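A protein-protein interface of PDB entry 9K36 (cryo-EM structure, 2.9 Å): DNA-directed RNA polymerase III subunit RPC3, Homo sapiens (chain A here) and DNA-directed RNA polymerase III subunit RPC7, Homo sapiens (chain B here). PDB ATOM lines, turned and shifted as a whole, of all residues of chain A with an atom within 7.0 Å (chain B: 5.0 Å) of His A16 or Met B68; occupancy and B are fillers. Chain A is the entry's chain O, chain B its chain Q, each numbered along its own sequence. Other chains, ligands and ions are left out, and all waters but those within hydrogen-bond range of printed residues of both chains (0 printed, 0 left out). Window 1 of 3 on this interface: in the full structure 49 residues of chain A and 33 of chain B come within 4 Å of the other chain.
The side-chain carboxylate (OE1) of Glu A513 lies within salt-bridge range of the guanidinium group (NH2) of Arg B65 (3.5 Å). The guanidinium group (NH1) of Arg A450 sits close to the guanidinium group (NH2) of Arg B65 (3.2 Å).
The side-chain carboxylate (OE1) of Glu A513 is in salt-bridge range of the guanidinium group (NH1) of Arg A450 (3.7 Å). The guanidinium group (NH2) of Arg A450 is in salt-bridge range of the side-chain carboxylate (OE1) of Glu A15. O of Leu A112 is in hydrogen-bond range of NE2 of His A60. O of Leu A13 is in hydrogen-bond range of N of Gly A18, at 3.1 Å. SD of Met A85 sits at hydrogen-bond distance from ND1 of His A16, 3.2 Å away.
Gln A14 touches Phe B74. Arg B65 touches Glu A15 (CD to OE2, 3.9 Å). Met B68 touches His A16. His A16 touches Phe B74 (O to CD1, 3.3 Å). Phe A17 touches Phe B74. Phe B74 touches Gly A18. Leu A112 touches Leu B64 (CD1 to CD2, 3.6 Å). CD2 of Leu A112 touches CG2 of Thr B67 (3.98 Å).
Of the printed residues of chain B, Glu A15 touches Arg B65 (3.9 Å). Of chain B, only Met B68 (3.1 Å) and Phe B74 (3.3 Å) come within 4 Å of His A16. Of the printed residues of chain B, Gly A18 touches Phe B74 (3.3 Å). Of the printed residues of chain B, Leu A112 touches Leu B64 (3.6 Å) and Thr B67 (3.98 Å). Printed residues of chain A within 4 Å of Arg B65: Glu A15, Arg A450 and Glu A513. Arg B70 touches none of the printed residues of chain A. Of the printed residues of chain A, Phe B74 touches Gln A14 (3.9 Å), His A16 (3.3 Å), Phe A17 (2.9 Å) and Gly A18 (3.3 Å). The nearest printed residue of chain B that does not touch His A16 is Lys B69 (5.1 Å). The nearest residue of chain A that does not touch Met B68 is Phe A17 (4.6 Å). The nearest printed residue of chain B that does not touch Gln A14 is Lys B69 (6.6 Å).
Of the 10 printed residues of chain B, 5 touch a printed residue of chain A. Hydrophobic or aromatic side chains of chain B within 4 Å of the printed part of chain A: Leu B64, Met B68 and Phe B74. Among the printed residues, 10 pairs touch across the chains. Among the printed residues, Asp or Glu carboxylates within 4 Å of a Lys or Arg side-chain nitrogen of the other chain: Glu A513 with Arg B65 (3.5 Å).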
ATOM      1  N   SER A  10      -9.670   2.839 -19.938  1.00  0.00           N
ATOM      2  CA  SER A  10      -8.315   2.434 -20.289  1.00  0.00           C
ATOM      3  C   SER A  10      -7.301   3.041 -19.330  1.00  0.00           C
ATOM      4  O   SER A  10      -6.403   2.348 -18.834  1.00  0.00           O
ATOM      5  CB  SER A  10      -8.002   2.845 -21.729  1.00  0.00           C
ATOM      6  OG  SER A  10      -6.684   2.468 -22.090  1.00  0.00           O
ATOM      7  N   LEU A  11      -7.430   4.343 -19.057  1.00  0.00           N
ATOM      8  CA  LEU A  11      -6.513   4.997 -18.128  1.00  0.00           C
ATOM      9  C   LEU A  11      -6.603   4.381 -16.737  1.00  0.00           C
ATOM     10  O   LEU A  11      -5.577   4.132 -16.092  1.00  0.00           O
ATOM     11  CB  LEU A  11      -6.802   6.497 -18.073  1.00  0.00           C
ATOM     12  CG  LEU A  11      -6.524   7.284 -19.356  1.00  0.00           C
ATOM     13  CD1 LEU A  11      -6.859   8.755 -19.160  1.00  0.00           C
ATOM     14  CD2 LEU A  11      -5.079   7.111 -19.789  1.00  0.00           C
ATOM     15  N   LEU A  12      -7.823   4.123 -16.259  1.00  0.00           N
ATOM     16  CA  LEU A  12      -7.991   3.551 -14.928  1.00  0.00           C
ATOM     17  C   LEU A  12      -7.394   2.151 -14.843  1.00  0.00           C
ATOM     18  O   LEU A  12      -6.699   1.822 -13.874  1.00  0.00           O
ATOM     19  CB  LEU A  12      -9.470   3.530 -14.545  1.00  0.00           C
ATOM     20  CG  LEU A  12     -10.120   4.887 -14.279  1.00  0.00           C
ATOM     21  CD1 LEU A  12     -11.582   4.716 -13.898  1.00  0.00           C
ATOM     22  CD2 LEU A  12      -9.364   5.639 -13.195  1.00  0.00           C
ATOM     23  N   LEU A  13      -7.653   1.312 -15.850  1.00  0.00           N
ATOM     24  CA  LEU A  13      -7.127  -0.051 -15.826  1.00  0.00           C
ATOM     25  C   LEU A  13      -5.610  -0.064 -15.971  1.00  0.00           C
ATOM     26  O   LEU A  13      -4.937  -0.931 -15.400  1.00  0.00           O
ATOM     27  CB  LEU A  13      -7.783  -0.883 -16.927  1.00  0.00           C
ATOM     28  CG  LEU A  13      -9.275  -1.174 -16.754  1.00  0.00           C
ATOM     29  CD1 LEU A  13      -9.794  -2.007 -17.913  1.00  0.00           C
ATOM     30  CD2 LEU A  13      -9.539  -1.868 -15.427  1.00  0.00           C
ATOM     31  N   GLN A  14      -5.049   0.884 -16.729  1.00  0.00           N
ATOM     32  CA  GLN A  14      -3.599   0.959 -16.853  1.00  0.00           C
ATOM     33  C   GLN A  14      -2.958   1.427 -15.556  1.00  0.00           C
ATOM     34  O   GLN A  14      -1.895   0.927 -15.165  1.00  0.00           O
ATOM     35  CB  GLN A  14      -3.220   1.886 -18.008  1.00  0.00           C
ATOM     36  CG  GLN A  14      -1.726   1.974 -18.274  1.00  0.00           C
ATOM     37  CD  GLN A  14      -1.396   2.887 -19.440  1.00  0.00           C
ATOM     38  OE1 GLN A  14      -2.289   3.464 -20.060  1.00  0.00           O
ATOM     39  NE2 GLN A  14      -0.113   3.025 -19.742  1.00  0.00           N
ATOM     40  N   GLU A  15      -3.588   2.383 -14.867  1.00  0.00           N
ATOM     41  CA  GLU A  15      -3.018   2.892 -13.626  1.00  0.00           C
ATOM     42  C   GLU A  15      -3.221   1.921 -12.467  1.00  0.00           C
ATOM     43  O   GLU A  15      -2.450   1.942 -11.500  1.00  0.00           O
ATOM     44  CB  GLU A  15      -3.626   4.256 -13.293  1.00  0.00           C
ATOM     45  CG  GLU A  15      -2.971   4.981 -12.125  1.00  0.00           C
ATOM     46  CD  GLU A  15      -1.569   5.460 -12.443  1.00  0.00           C
ATOM     47  OE1 GLU A  15      -1.239   5.601 -13.639  1.00  0.00           O
ATOM     48  OE2 GLU A  15      -0.792   5.694 -11.493  1.00  0.00           O
ATOM     49  N   HIS A  16      -4.236   1.061 -12.545  1.00  0.00           N
ATOM     50  CA  HIS A  16      -4.609   0.213 -11.423  1.00  0.00           C
ATOM     51  C   HIS A  16      -4.217  -1.250 -11.578  1.00  0.00           C
ATOM     52  O   HIS A  16      -3.942  -1.904 -10.572  1.00  0.00           O
ATOM     53  CB  HIS A  16      -6.123   0.287 -11.185  1.00  0.00           C
ATOM     54  CG  HIS A  16      -6.601   1.635 -10.742  1.00  0.00           C
ATOM     55  ND1 HIS A  16      -7.934   1.915 -10.520  1.00  0.00           N
ATOM     56  CD2 HIS A  16      -5.928   2.777 -10.472  1.00  0.00           C
ATOM     57  CE1 HIS A  16      -8.057   3.173 -10.136  1.00  0.00           C
ATOM     58  NE2 HIS A  16      -6.857   3.718 -10.098  1.00  0.00           N
ATOM     59  N   PHE A  17      -4.180  -1.781 -12.799  1.00  0.00           N
ATOM     60  CA  PHE A  17      -3.992  -3.220 -12.963  1.00  0.00           C
ATOM     61  C   PHE A  17      -2.776  -3.564 -13.814  1.00  0.00           C
ATOM     62  O   PHE A  17      -2.116  -4.580 -13.565  1.00  0.00           O
ATOM     63  CB  PHE A  17      -5.253  -3.846 -13.565  1.00  0.00           C
ATOM     64  CG  PHE A  17      -6.393  -3.957 -12.593  1.00  0.00           C
ATOM     65  CD1 PHE A  17      -6.152  -4.078 -11.235  1.00  0.00           C
ATOM     66  CD2 PHE A  17      -7.703  -3.938 -13.036  1.00  0.00           C
ATOM     67  CE1 PHE A  17      -7.196  -4.180 -10.337  1.00  0.00           C
ATOM     68  CE2 PHE A  17      -8.752  -4.040 -12.142  1.00  0.00           C
ATOM     69  CZ  PHE A  17      -8.500  -4.161 -10.792  1.00  0.00           C
ATOM     70  N   GLY A  18      -2.464  -2.745 -14.815  1.00  0.00           N
ATOM     71  CA  GLY A  18      -1.310  -2.991 -15.648  1.00  0.00           C
ATOM     72  C   GLY A  18      -1.629  -2.765 -17.109  1.00  0.00           C
ATOM     73  O   GLY A  18      -2.608  -2.097 -17.458  1.00  0.00           O
ATOM     74  N   VAL A  21      -3.506  -6.398 -19.101  1.00  0.00           N
ATOM     75  CA  VAL A  21      -4.888  -6.591 -18.673  1.00  0.00           C
ATOM     76  C   VAL A  21      -5.781  -5.452 -19.149  1.00  0.00           C
ATOM     77  O   VAL A  21      -6.952  -5.669 -19.481  1.00  0.00           O
ATOM     78  CB  VAL A  21      -4.934  -6.757 -17.139  1.00  0.00           C
ATOM     79  CG1 VAL A  21      -4.142  -5.650 -16.461  1.00  0.00           C
ATOM     80  CG2 VAL A  21      -6.372  -6.786 -16.637  1.00  0.00           C
ATOM     81  N   HIS A  60     -12.355  -8.817  -9.524  1.00  0.00           N
ATOM     82  CA  HIS A  60     -12.845  -7.523  -9.069  1.00  0.00           C
ATOM     83  C   HIS A  60     -14.250  -7.214  -9.576  1.00  0.00           C
ATOM     84  O   HIS A  60     -14.672  -6.054  -9.512  1.00  0.00           O
ATOM     85  CB  HIS A  60     -11.881  -6.411  -9.496  1.00  0.00           C
ATOM     86  CG  HIS A  60     -10.534  -6.496  -8.848  1.00  0.00           C
ATOM     87  ND1 HIS A  60      -9.652  -7.525  -9.094  1.00  0.00           N
ATOM     88  CD2 HIS A  60      -9.920  -5.678  -7.962  1.00  0.00           C
ATOM     89  CE1 HIS A  60      -8.551  -7.337  -8.388  1.00  0.00           C
ATOM     90  NE2 HIS A  60      -8.687  -6.222  -7.691  1.00  0.00           N
ATOM     91  N   VAL A  82     -16.296  -0.259 -14.089  1.00  0.00           N
ATOM     92  CA  VAL A  82     -14.979   0.353 -14.239  1.00  0.00           C
ATOM     93  C   VAL A  82     -15.057   1.850 -13.955  1.00  0.00           C
ATOM     94  O   VAL A  82     -14.104   2.447 -13.439  1.00  0.00           O
ATOM     95  CB  VAL A  82     -14.408   0.070 -15.640  1.00  0.00           C
ATOM     96  CG1 VAL A  82     -12.962   0.538 -15.730  1.00  0.00           C
ATOM     97  CG2 VAL A  82     -14.513  -1.412 -15.963  1.00  0.00           C
ATOM     98  N   MET A  85     -15.282   2.303 -10.223  1.00  0.00           N
ATOM     99  CA  MET A  85     -13.989   2.059  -9.587  1.00  0.00           C
ATOM    100  C   MET A  85     -13.325   3.357  -9.135  1.00  0.00           C
ATOM    101  O   MET A  85     -12.613   3.373  -8.125  1.00  0.00           O
ATOM    102  CB  MET A  85     -13.075   1.295 -10.544  1.00  0.00           C
ATOM    103  CG  MET A  85     -11.640   1.139 -10.062  1.00  0.00           C
ATOM    104  SD  MET A  85     -10.586   0.249 -11.226  1.00  0.00           S
ATOM    105  CE  MET A  85     -11.346  -1.372 -11.205  1.00  0.00           C
ATOM    106  N   LEU A  86     -13.551   4.456  -9.863  1.00  0.00           N
ATOM    107  CA  LEU A  86     -12.973   5.740  -9.489  1.00  0.00           C
ATOM    108  C   LEU A  86     -13.534   6.272  -8.175  1.00  0.00           C
ATOM    109  O   LEU A  86     -12.873   7.081  -7.517  1.00  0.00           O
ATOM    110  CB  LEU A  86     -13.204   6.756 -10.610  1.00  0.00           C
ATOM    111  CG  LEU A  86     -12.569   8.138 -10.461  1.00  0.00           C
ATOM    112  CD1 LEU A  86     -11.066   8.010 -10.269  1.00  0.00           C
ATOM    113  CD2 LEU A  86     -12.887   9.008 -11.667  1.00  0.00           C
ATOM    114  N   TYR A  88     -13.803   4.822  -5.397  1.00  0.00           N
ATOM    115  CA  TYR A  88     -13.298   4.116  -4.219  1.00  0.00           C
ATOM    116  C   TYR A  88     -12.908   5.053  -3.081  1.00  0.00           C
ATOM    117  O   TYR A  88     -13.282   4.772  -1.930  1.00  0.00           O
ATOM    118  CB  TYR A  88     -12.130   3.207  -4.615  1.00  0.00           C
ATOM    119  CG  TYR A  88     -12.525   1.984  -5.414  1.00  0.00           C
ATOM    120  CD1 TYR A  88     -13.861   1.644  -5.589  1.00  0.00           C
ATOM    121  CD2 TYR A  88     -11.560   1.166  -5.984  1.00  0.00           C
ATOM    122  CE1 TYR A  88     -14.224   0.527  -6.317  1.00  0.00           C
ATOM    123  CE2 TYR A  88     -11.912   0.045  -6.712  1.00  0.00           C
ATOM    124  CZ  TYR A  88     -13.246  -0.271  -6.875  1.00  0.00           C
ATOM    125  OH  TYR A  88     -13.601  -1.385  -7.599  1.00  0.00           O
ATOM    126  N   LEU A 111     -12.672  -3.536  -1.554  1.00  0.00           N
ATOM    127  CA  LEU A 111     -12.512  -2.869  -2.842  1.00  0.00           C
ATOM    128  C   LEU A 111     -11.190  -3.240  -3.503  1.00  0.00           C
ATOM    129  O   LEU A 111     -11.109  -3.334  -4.733  1.00  0.00           O
ATOM    130  CB  LEU A 111     -12.624  -1.355  -2.666  1.00  0.00           C
ATOM    131  CG  LEU A 111     -14.013  -0.829  -2.299  1.00  0.00           C
ATOM    132  CD1 LEU A 111     -13.995   0.685  -2.154  1.00  0.00           C
ATOM    133  CD2 LEU A 111     -15.040  -1.259  -3.334  1.00  0.00           C
ATOM    134  N   LEU A 112     -10.139  -3.455  -2.705  1.00  0.00           N
ATOM    135  CA  LEU A 112      -8.840  -3.799  -3.269  1.00  0.00           C
ATOM    136  C   LEU A 112      -8.755  -5.260  -3.696  1.00  0.00           C
ATOM    137  O   LEU A 112      -7.898  -5.600  -4.521  1.00  0.00           O
ATOM    138  CB  LEU A 112      -7.727  -3.485  -2.269  1.00  0.00           C
ATOM    139  CG  LEU A 112      -7.048  -2.119  -2.391  1.00  0.00           C
ATOM    140  CD1 LEU A 112      -8.053  -0.982  -2.274  1.00  0.00           C
ATOM    141  CD2 LEU A 112      -5.946  -1.973  -1.353  1.00  0.00           C
ATOM    142  N   ARG A 450      -1.509  14.138 -15.302  1.00  0.00           N
ATOM    143  CA  ARG A 450      -0.785  13.627 -14.143  1.00  0.00           C
ATOM    144  C   ARG A 450       0.244  12.581 -14.556  1.00  0.00           C
ATOM    145  O   ARG A 450       1.386  12.603 -14.086  1.00  0.00           O
ATOM    146  CB  ARG A 450      -1.760  13.036 -13.123  1.00  0.00           C
ATOM    147  CG  ARG A 450      -1.103  12.678 -11.795  1.00  0.00           C
ATOM    148  CD  ARG A 450      -1.959  11.730 -10.971  1.00  0.00           C
ATOM    149  NE  ARG A 450      -1.974  10.377 -11.522  1.00  0.00           N
ATOM    150  CZ  ARG A 450      -2.958   9.881 -12.265  1.00  0.00           C
ATOM    151  NH1 ARG A 450      -4.018  10.626 -12.549  1.00  0.00           N
ATOM    152  NH2 ARG A 450      -2.883   8.639 -12.723  1.00  0.00           N
ATOM    153  N   GLU A 513      -9.769  15.690  -9.816  1.00  0.00           N
ATOM    154  CA  GLU A 513     -10.323  14.443 -10.332  1.00  0.00           C
ATOM    155  C   GLU A 513     -11.336  13.846  -9.364  1.00  0.00           C
ATOM    156  O   GLU A 513     -12.353  13.281  -9.783  1.00  0.00           O
ATOM    157  CB  GLU A 513      -9.192  13.453 -10.611  1.00  0.00           C
ATOM    158  CG  GLU A 513      -9.648  12.074 -11.056  1.00  0.00           C
ATOM    159  CD  GLU A 513      -8.484  11.126 -11.287  1.00  0.00           C
ATOM    160  OE1 GLU A 513      -7.325  11.589 -11.258  1.00  0.00           O
ATOM    161  OE2 GLU A 513      -8.730   9.922 -11.494  1.00  0.00           O
ATOM    162  N   GLU B  63      -2.406   6.768  -1.522  1.00  0.00           N
ATOM    163  CA  GLU B  63      -2.048   5.500  -0.897  1.00  0.00           C
ATOM    164  C   GLU B  63      -2.526   4.316  -1.731  1.00  0.00           C
ATOM    165  O   GLU B  63      -1.817   3.313  -1.857  1.00  0.00           O
ATOM    166  CB  GLU B  63      -2.628   5.427   0.516  1.00  0.00           C
ATOM    167  CG  GLU B  63      -1.971   6.370   1.510  1.00  0.00           C
ATOM    168  CD  GLU B  63      -2.602   6.299   2.885  1.00  0.00           C
ATOM    169  OE1 GLU B  63      -3.564   5.523   3.063  1.00  0.00           O
ATOM    170  OE2 GLU B  63      -2.133   7.019   3.793  1.00  0.00           O
ATOM    171  N   LEU B  64      -3.725   4.417  -2.305  1.00  0.00           N
ATOM    172  CA  LEU B  64      -4.225   3.349  -3.166  1.00  0.00           C
ATOM    173  C   LEU B  64      -3.372   3.211  -4.420  1.00  0.00           C
ATOM    174  O   LEU B  64      -3.057   2.094  -4.845  1.00  0.00           O
ATOM    175  CB  LEU B  64      -5.687   3.601  -3.536  1.00  0.00           C
ATOM    176  CG  LEU B  64      -6.707   3.520  -2.398  1.00  0.00           C
ATOM    177  CD1 LEU B  64      -8.122   3.662  -2.934  1.00  0.00           C
ATOM    178  CD2 LEU B  64      -6.547   2.222  -1.621  1.00  0.00           C
ATOM    179  N   ARG B  65      -2.998   4.338  -5.032  1.00  0.00           N
ATOM    180  CA  ARG B  65      -2.095   4.297  -6.178  1.00  0.00           C
ATOM    181  C   ARG B  65      -0.787   3.604  -5.819  1.00  0.00           C
ATOM    182  O   ARG B  65      -0.255   2.807  -6.602  1.00  0.00           O
ATOM    183  CB  ARG B  65      -1.820   5.711  -6.692  1.00  0.00           C
ATOM    184  CG  ARG B  65      -2.911   6.303  -7.565  1.00  0.00           C
ATOM    185  CD  ARG B  65      -2.339   7.425  -8.419  1.00  0.00           C
ATOM    186  NE  ARG B  65      -3.362   8.125  -9.193  1.00  0.00           N
ATOM    187  CZ  ARG B  65      -3.909   9.278  -8.829  1.00  0.00           C
ATOM    188  NH1 ARG B  65      -3.534   9.862  -7.699  1.00  0.00           N
ATOM    189  NH2 ARG B  65      -4.829   9.847  -9.592  1.00  0.00           N
ATOM    190  N   GLU B  66      -0.250   3.899  -4.632  1.00  0.00           N
ATOM    191  CA  GLU B  66       1.034   3.317  -4.246  1.00  0.00           C
ATOM    192  C   GLU B  66       0.914   1.840  -3.884  1.00  0.00           C
ATOM    193  O   GLU B  66       1.861   1.077  -4.098  1.00  0.00           O
ATOM    194  CB  GLU B  66       1.633   4.099  -3.076  1.00  0.00           C
ATOM    195  CG  GLU B  66       2.020   5.527  -3.414  1.00  0.00           C
ATOM    196  CD  GLU B  66       2.635   6.259  -2.238  1.00  0.00           C
ATOM    197  OE1 GLU B  66       2.742   5.656  -1.152  1.00  0.00           O
ATOM    198  OE2 GLU B  66       3.018   7.438  -2.404  1.00  0.00           O
ATOM    199  N   THR B  67      -0.229   1.417  -3.344  1.00  0.00           N
ATOM    200  CA  THR B  67      -0.356   0.057  -2.835  1.00  0.00           C
ATOM    201  C   THR B  67      -0.953  -0.916  -3.843  1.00  0.00           C
ATOM    202  O   THR B  67      -0.801  -2.133  -3.673  1.00  0.00           O
ATOM    203  CB  THR B  67      -1.202   0.041  -1.557  1.00  0.00           C
ATOM    204  OG1 THR B  67      -1.034  -1.215  -0.886  1.00  0.00           O
ATOM    205  CG2 THR B  67      -2.677   0.233  -1.883  1.00  0.00           C
ATOM    206  N   MET B  68      -1.624  -0.428  -4.886  1.00  0.00           N
ATOM    207  CA  MET B  68      -2.265  -1.315  -5.844  1.00  0.00           C
ATOM    208  C   MET B  68      -1.334  -1.758  -6.965  1.00  0.00           C
ATOM    209  O   MET B  68      -1.631  -2.751  -7.639  1.00  0.00           O
ATOM    210  CB  MET B  68      -3.508  -0.633  -6.432  1.00  0.00           C
ATOM    211  CG  MET B  68      -4.470  -1.574  -7.142  1.00  0.00           C
ATOM    212  SD  MET B  68      -6.140  -0.906  -7.237  1.00  0.00           S
ATOM    213  CE  MET B  68      -5.816   0.726  -7.897  1.00  0.00           C
ATOM    214  N   LYS B  69      -0.214  -1.064  -7.173  1.00  0.00           N
ATOM    215  CA  LYS B  69       0.747  -1.505  -8.177  1.00  0.00           C
ATOM    216  C   LYS B  69       1.555  -2.700  -7.685  1.00  0.00           C
ATOM    217  O   LYS B  69       1.913  -3.580  -8.478  1.00  0.00           O
ATOM    218  CB  LYS B  69       1.676  -0.353  -8.560  1.00  0.00           C
ATOM    219  CG  LYS B  69       0.960   0.842  -9.176  1.00  0.00           C
ATOM    220  CD  LYS B  69       1.951   1.854  -9.725  1.00  0.00           C
ATOM    221  CE  LYS B  69       2.914   2.328  -8.648  1.00  0.00           C
ATOM    222  NZ  LYS B  69       3.909   3.300  -9.179  1.00  0.00           N
ATOM    223  N   ARG B  70       1.852  -2.748  -6.387  1.00  0.00           N
ATOM    224  CA  ARG B  70       2.528  -3.894  -5.797  1.00  0.00           C
ATOM    225  C   ARG B  70       1.579  -5.047  -5.494  1.00  0.00           C
ATOM    226  O   ARG B  70       2.045  -6.123  -5.106  1.00  0.00           O
ATOM    227  CB  ARG B  70       3.260  -3.475  -4.520  1.00  0.00           C
ATOM    228  CG  ARG B  70       4.437  -2.540  -4.759  1.00  0.00           C
ATOM    229  CD  ARG B  70       5.053  -2.052  -3.453  1.00  0.00           C
ATOM    230  NE  ARG B  70       4.231  -1.038  -2.795  1.00  0.00           N
ATOM    231  CZ  ARG B  70       3.389  -1.283  -1.796  1.00  0.00           C
ATOM    232  NH1 ARG B  70       3.251  -2.517  -1.330  1.00  0.00           N
ATOM    233  NH2 ARG B  70       2.685  -0.294  -1.261  1.00  0.00           N
ATOM    234  N   MET B  71       0.277  -4.846  -5.654  1.00  0.00           N
ATOM    235  CA  MET B  71      -0.678  -5.922  -5.432  1.00  0.00           C
ATOM    236  C   MET B  71      -0.510  -6.988  -6.513  1.00  0.00           C
ATOM    237  O   MET B  71      -0.261  -6.656  -7.678  1.00  0.00           O
ATOM    238  CB  MET B  71      -2.106  -5.375  -5.443  1.00  0.00           C
ATOM    239  CG  MET B  71      -3.151  -6.319  -4.875  1.00  0.00           C
ATOM    240  SD  MET B  71      -2.925  -6.624  -3.112  1.00  0.00           S
ATOM    241  CE  MET B  71      -4.237  -7.802  -2.804  1.00  0.00           C
ATOM    242  N   PHE B  74      -2.121  -6.519  -9.934  1.00  0.00           N
ATOM    243  CA  PHE B  74      -1.436  -5.689 -10.922  1.00  0.00           C
ATOM    244  C   PHE B  74      -0.401  -6.543 -11.637  1.00  0.00           C
ATOM    245  O   PHE B  74       0.729  -6.696 -11.168  1.00  0.00           O
ATOM    246  CB  PHE B  74      -0.791  -4.482 -10.245  1.00  0.00           C
ATOM    247  CG  PHE B  74      -0.158  -3.512 -11.204  1.00  0.00           C
ATOM    248  CD1 PHE B  74      -0.897  -2.470 -11.744  1.00  0.00           C
ATOM    249  CD2 PHE B  74       1.177  -3.630 -11.556  1.00  0.00           C
ATOM    250  CE1 PHE B  74      -0.319  -1.573 -12.624  1.00  0.00           C
ATOM    251  CE2 PHE B  74       1.761  -2.736 -12.437  1.00  0.00           C
ATOM    252  CZ  PHE B  74       1.010  -1.707 -12.969  1.00  0.00           C
